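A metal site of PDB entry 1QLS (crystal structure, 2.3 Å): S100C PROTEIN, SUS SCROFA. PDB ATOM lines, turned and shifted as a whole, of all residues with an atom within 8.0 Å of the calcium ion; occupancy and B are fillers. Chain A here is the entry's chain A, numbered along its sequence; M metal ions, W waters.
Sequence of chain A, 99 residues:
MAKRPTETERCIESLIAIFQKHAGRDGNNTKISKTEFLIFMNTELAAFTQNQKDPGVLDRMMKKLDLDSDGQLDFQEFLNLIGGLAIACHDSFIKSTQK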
ATOM      1  N   PHE A  19      -1.742   5.167 -14.068  1.00  0.00           N
ATOM      2  CA  PHE A  19      -2.525   5.243 -12.831  1.00  0.00           C
ATOM      3  C   PHE A  19      -2.453   3.935 -12.054  1.00  0.00           C
ATOM      4  O   PHE A  19      -2.199   3.907 -10.847  1.00  0.00           O
ATOM      5  CB  PHE A  19      -3.980   5.533 -13.131  1.00  0.00           C
ATOM      6  CG  PHE A  19      -4.839   5.547 -11.926  1.00  0.00           C
ATOM      7  CD1 PHE A  19      -4.900   6.692 -11.127  1.00  0.00           C
ATOM      8  CD2 PHE A  19      -5.615   4.422 -11.558  1.00  0.00           C
ATOM      9  CE1 PHE A  19      -5.675   6.754 -10.014  1.00  0.00           C
ATOM     10  CE2 PHE A  19      -6.402   4.477 -10.434  1.00  0.00           C
ATOM     11  CZ  PHE A  19      -6.451   5.629  -9.646  1.00  0.00           C
ATOM     12  N   GLN A  20      -2.649   2.841 -12.732  1.00  0.00           N
ATOM     13  CA  GLN A  20      -2.695   1.509 -12.142  1.00  0.00           C
ATOM     14  C   GLN A  20      -1.420   1.057 -11.515  1.00  0.00           C
ATOM     15  O   GLN A  20      -1.356   0.504 -10.392  1.00  0.00           O
ATOM     16  CB  GLN A  20      -3.288   0.525 -13.185  1.00  0.00           C
ATOM     17  CG  GLN A  20      -4.600  -0.061 -12.650  1.00  0.00           C
ATOM     18  CD  GLN A  20      -5.788   0.813 -12.433  1.00  0.00           C
ATOM     19  OE1 GLN A  20      -6.098   1.737 -13.220  1.00  0.00           O
ATOM     20  NE2 GLN A  20      -6.562   0.612 -11.383  1.00  0.00           N
ATOM     21  N   LYS A  21      -0.301   1.364 -12.147  1.00  0.00           N
ATOM     22  CA  LYS A  21       1.009   1.088 -11.592  1.00  0.00           C
ATOM     23  C   LYS A  21       1.222   1.896 -10.289  1.00  0.00           C
ATOM     24  O   LYS A  21       1.764   1.340  -9.312  1.00  0.00           O
ATOM     25  CB  LYS A  21       2.091   1.592 -12.542  1.00  0.00           C
ATOM     26  CG  LYS A  21       3.495   1.280 -11.949  1.00  0.00           C
ATOM     27  CD  LYS A  21       4.521   1.753 -12.956  1.00  0.00           C
ATOM     28  CE  LYS A  21       5.901   1.979 -12.353  1.00  0.00           C
ATOM     29  NZ  LYS A  21       6.724   2.829 -13.288  1.00  0.00           N
ATOM     30  N   HIS A  22       0.841   3.164 -10.295  1.00  0.00           N
ATOM     31  CA  HIS A  22       1.061   3.962  -9.080  1.00  0.00           C
ATOM     32  C   HIS A  22      -0.009   3.721  -8.048  1.00  0.00           C
ATOM     33  O   HIS A  22       0.243   3.775  -6.846  1.00  0.00           O
ATOM     34  CB  HIS A  22       1.162   5.470  -9.402  1.00  0.00           C
ATOM     35  CG  HIS A  22       2.501   5.653 -10.111  1.00  0.00           C
ATOM     36  ND1 HIS A  22       2.598   5.541 -11.498  1.00  0.00           N
ATOM     37  CD2 HIS A  22       3.732   5.891  -9.633  1.00  0.00           C
ATOM     38  CE1 HIS A  22       3.858   5.723 -11.852  1.00  0.00           C
ATOM     39  NE2 HIS A  22       4.560   5.943 -10.739  1.00  0.00           N
ATOM     40  N   ALA A  23      -1.244   3.380  -8.531  1.00  0.00           N
ATOM     41  CA  ALA A  23      -2.271   3.121  -7.519  1.00  0.00           C
ATOM     42  C   ALA A  23      -2.072   1.728  -6.971  1.00  0.00           C
ATOM     43  O   ALA A  23      -2.585   1.484  -5.889  1.00  0.00           O
ATOM     44  CB  ALA A  23      -3.679   3.162  -8.085  1.00  0.00           C
ATOM     45  N   GLY A  24      -1.431   0.764  -7.577  1.00  0.00           N
ATOM     46  CA  GLY A  24      -1.338  -0.568  -7.025  1.00  0.00           C
ATOM     47  C   GLY A  24      -0.188  -0.844  -6.114  1.00  0.00           C
ATOM     48  O   GLY A  24       0.094  -2.027  -5.967  1.00  0.00           O
ATOM     49  N   ARG A  25       0.401   0.139  -5.404  1.00  0.00           N
ATOM     50  CA  ARG A  25       1.488  -0.213  -4.513  1.00  0.00           C
ATOM     51  C   ARG A  25       0.891  -0.692  -3.179  1.00  0.00           C
ATOM     52  O   ARG A  25       1.519  -1.510  -2.543  1.00  0.00           O
ATOM     53  CB  ARG A  25       2.393   0.979  -4.134  1.00  0.00           C
ATOM     54  CG  ARG A  25       2.913   1.888  -5.184  1.00  0.00           C
ATOM     55  CD  ARG A  25       3.635   1.171  -6.323  1.00  0.00           C
ATOM     56  NE  ARG A  25       4.229   2.245  -7.173  1.00  0.00           N
ATOM     57  CZ  ARG A  25       5.495   2.633  -7.171  1.00  0.00           C
ATOM     58  NH1 ARG A  25       6.415   2.091  -6.386  1.00  0.00           N
ATOM     59  NH2 ARG A  25       5.828   3.610  -7.985  1.00  0.00           N
ATOM     60  N   ASP A  26      -0.224  -0.130  -2.723  1.00  0.00           N
ATOM     61  CA  ASP A  26      -0.752  -0.622  -1.461  1.00  0.00           C
ATOM     62  C   ASP A  26      -1.894  -1.626  -1.795  1.00  0.00           C
ATOM     63  O   ASP A  26      -1.946  -2.147  -2.930  1.00  0.00           O
ATOM     64  CB  ASP A  26      -1.143   0.500  -0.535  1.00  0.00           C
ATOM     65  CG  ASP A  26      -2.243   1.368  -1.025  1.00  0.00           C
ATOM     66  OD1 ASP A  26      -2.788   0.937  -2.092  1.00  0.00           O
ATOM     67  OD2 ASP A  26      -2.726   2.409  -0.553  1.00  0.00           O
ATOM     68  N   GLY A  27      -2.814  -1.914  -0.863  1.00  0.00           N
ATOM     69  CA  GLY A  27      -3.862  -2.896  -1.177  1.00  0.00           C
ATOM     70  C   GLY A  27      -5.083  -2.409  -1.906  1.00  0.00           C
ATOM     71  O   GLY A  27      -6.062  -3.139  -2.033  1.00  0.00           O
ATOM     72  N   ASN A  28      -5.083  -1.125  -2.323  1.00  0.00           N
ATOM     73  CA  ASN A  28      -6.229  -0.597  -3.040  1.00  0.00           C
ATOM     74  C   ASN A  28      -5.842  -0.159  -4.405  1.00  0.00           C
ATOM     75  O   ASN A  28      -5.514   0.994  -4.564  1.00  0.00           O
ATOM     76  CB  ASN A  28      -6.868   0.524  -2.229  1.00  0.00           C
ATOM     77  CG  ASN A  28      -8.105   1.100  -2.840  1.00  0.00           C
ATOM     78  OD1 ASN A  28      -8.516   0.768  -3.952  1.00  0.00           O
ATOM     79  ND2 ASN A  28      -8.742   1.982  -2.092  1.00  0.00           N
ATOM     80  N   ASN A  29      -5.932  -0.881  -5.515  1.00  0.00           N
ATOM     81  CA  ASN A  29      -5.487  -0.264  -6.783  1.00  0.00           C
ATOM     82  C   ASN A  29      -6.477   0.595  -7.436  1.00  0.00           C
ATOM     83  O   ASN A  29      -6.291   0.843  -8.655  1.00  0.00           O
ATOM     84  CB  ASN A  29      -5.027  -1.374  -7.722  1.00  0.00           C
ATOM     85  CG  ASN A  29      -6.229  -2.309  -8.028  1.00  0.00           C
ATOM     86  OD1 ASN A  29      -5.948  -3.343  -8.637  1.00  0.00           O
ATOM     87  ND2 ASN A  29      -7.432  -2.053  -7.644  1.00  0.00           N
ATOM     88  N   THR A  30      -7.492   1.130  -6.791  1.00  0.00           N
ATOM     89  CA  THR A  30      -8.395   2.012  -7.502  1.00  0.00           C
ATOM     90  C   THR A  30      -8.215   3.420  -6.951  1.00  0.00           C
ATOM     91  O   THR A  30      -8.887   4.367  -7.383  1.00  0.00           O
ATOM     92  CB  THR A  30      -9.908   1.617  -7.300  1.00  0.00           C
ATOM     93  OG1 THR A  30     -10.207   1.863  -5.928  1.00  0.00           O
ATOM     94  CG2 THR A  30     -10.134   0.125  -7.593  1.00  0.00           C
ATOM     95  N   LYS A  31      -7.259   3.565  -6.004  1.00  0.00           N
ATOM     96  CA  LYS A  31      -7.098   4.942  -5.427  1.00  0.00           C
ATOM     97  C   LYS A  31      -5.648   5.342  -5.298  1.00  0.00           C
ATOM     98  O   LYS A  31      -4.822   4.446  -5.044  1.00  0.00           O
ATOM     99  CB  LYS A  31      -7.798   4.930  -4.026  1.00  0.00           C
ATOM    100  CG  LYS A  31      -9.224   5.525  -4.262  1.00  0.00           C
ATOM    101  CD  LYS A  31      -9.924   5.600  -2.933  1.00  0.00           C
ATOM    102  CE  LYS A  31     -11.444   5.865  -3.136  1.00  0.00           C
ATOM    103  NZ  LYS A  31     -11.706   5.835  -4.600  1.00  0.00           N
ATOM    104  N   ILE A  32      -5.188   6.553  -5.592  1.00  0.00           N
ATOM    105  CA  ILE A  32      -3.738   6.790  -5.349  1.00  0.00           C
ATOM    106  C   ILE A  32      -3.656   7.383  -3.978  1.00  0.00           C
ATOM    107  O   ILE A  32      -4.349   8.429  -3.721  1.00  0.00           O
ATOM    108  CB  ILE A  32      -3.217   7.744  -6.469  1.00  0.00           C
ATOM    109  CG1 ILE A  32      -2.817   6.887  -7.669  1.00  0.00           C
ATOM    110  CG2 ILE A  32      -1.938   8.502  -5.997  1.00  0.00           C
ATOM    111  CD1 ILE A  32      -2.410   7.672  -8.899  1.00  0.00           C
ATOM    112  N   SER A  33      -2.980   6.750  -2.986  1.00  0.00           N
ATOM    113  CA  SER A  33      -2.980   7.512  -1.692  1.00  0.00           C
ATOM    114  C   SER A  33      -1.918   8.684  -1.736  1.00  0.00           C
ATOM    115  O   SER A  33      -1.200   8.892  -2.733  1.00  0.00           O
ATOM    116  CB  SER A  33      -2.494   6.524  -0.617  1.00  0.00           C
ATOM    117  OG  SER A  33      -1.119   6.220  -0.913  1.00  0.00           O
ATOM    118  N   LYS A  34      -1.799   9.435  -0.678  1.00  0.00           N
ATOM    119  CA  LYS A  34      -0.840  10.546  -0.516  1.00  0.00           C
ATOM    120  C   LYS A  34       0.583  10.044  -0.716  1.00  0.00           C
ATOM    121  O   LYS A  34       1.322  10.559  -1.530  1.00  0.00           O
ATOM    122  CB  LYS A  34      -0.936  11.118   0.894  1.00  0.00           C
ATOM    123  CG  LYS A  34       0.197  12.098   1.195  1.00  0.00           C
ATOM    124  CD  LYS A  34      -0.322  13.539   1.129  1.00  0.00           C
ATOM    125  CE  LYS A  34      -0.339  14.123   2.545  1.00  0.00           C
ATOM    126  NZ  LYS A  34      -0.665  15.590   2.520  1.00  0.00           N
ATOM    127  N   GLU A  36       1.562   7.383  -2.430  1.00  0.00           N
ATOM    128  CA  GLU A  36       1.702   7.007  -3.810  1.00  0.00           C
ATOM    129  C   GLU A  36       1.702   8.244  -4.701  1.00  0.00           C
ATOM    130  O   GLU A  36       2.321   8.119  -5.733  1.00  0.00           O
ATOM    131  CB  GLU A  36       0.473   6.156  -4.297  1.00  0.00           C
ATOM    132  CG  GLU A  36       0.634   4.747  -3.769  1.00  0.00           C
ATOM    133  CD  GLU A  36      -0.714   3.982  -3.752  1.00  0.00           C
ATOM    134  OE1 GLU A  36      -1.782   4.611  -3.841  1.00  0.00           O
ATOM    135  OE2 GLU A  36      -0.682   2.758  -3.614  1.00  0.00           O
ATOM    136  N   GLN A  72      -7.654  10.533  -1.036  1.00  0.00           N
ATOM    137  CA  GLN A  72      -6.896   9.685  -1.997  1.00  0.00           C
ATOM    138  C   GLN A  72      -7.170  10.142  -3.398  1.00  0.00           C
ATOM    139  O   GLN A  72      -8.090  10.946  -3.463  1.00  0.00           O
ATOM    140  CB  GLN A  72      -7.357   8.218  -1.842  1.00  0.00           C
ATOM    141  CG  GLN A  72      -6.866   7.646  -0.491  1.00  0.00           C
ATOM    142  CD  GLN A  72      -6.681   6.173  -0.555  1.00  0.00           C
ATOM    143  OE1 GLN A  72      -5.716   5.730  -1.186  1.00  0.00           O
ATOM    144  NE2 GLN A  72      -7.567   5.403   0.080  1.00  0.00           N
ATOM    145  N   LEU A  73      -6.538   9.838  -4.500  1.00  0.00           N
ATOM    146  CA  LEU A  73      -6.994  10.386  -5.769  1.00  0.00           C
ATOM    147  C   LEU A  73      -7.611   9.167  -6.508  1.00  0.00           C
ATOM    148  O   LEU A  73      -6.959   8.114  -6.562  1.00  0.00           O
ATOM    149  CB  LEU A  73      -5.855  10.928  -6.647  1.00  0.00           C
ATOM    150  CG  LEU A  73      -5.038  12.099  -6.012  1.00  0.00           C
ATOM    151  CD1 LEU A  73      -3.960  12.652  -6.935  1.00  0.00           C
ATOM    152  CD2 LEU A  73      -5.942  13.228  -5.595  1.00  0.00           C
HETATM  153 CA    CA M   1      -3.488   2.613  -3.870  1.00  0.00          CA
HETATM  154  O   HOH W   1      -4.626   3.616  -1.894  1.00  0.00           O
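The backbone NH (N) of Glu 36 lies within hydrogen-bond range of the side-chain hydroxyl (OG) of Ser 33 (3.3 Å).
The side-chain carboxylate of Glu 36 sits close to the backbone NH of Arg 25.
OD1 of Asn 28 lies within hydrogen-bond range of OG1 of Thr 30 (2.8 Å).
The calcium ion is bound by the backbone carbonyl oxygen (O) of Ala 23 (2.5 Å).
Water W1 binds the calcium ion (2.5 Å).
OD1 of Asp 26 binds the calcium ion (2.5 Å).
O of Lys 31 is bound to the calcium ion, 2.6 Å away.
The side-chain carboxylate (OE1) of Glu 36 is bound to the calcium ion, 2.6 Å away.
The calcium ion is bound by O of Asn 28 (2.7 Å).
The side-chain carboxylate (OE2) of Glu 36 is bound to the calcium ion (2.8 Å).
Water W1 bridges OE1 of Gln 72 (2.5 Å) and OD2 of Asp 26 (2.6 Å).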
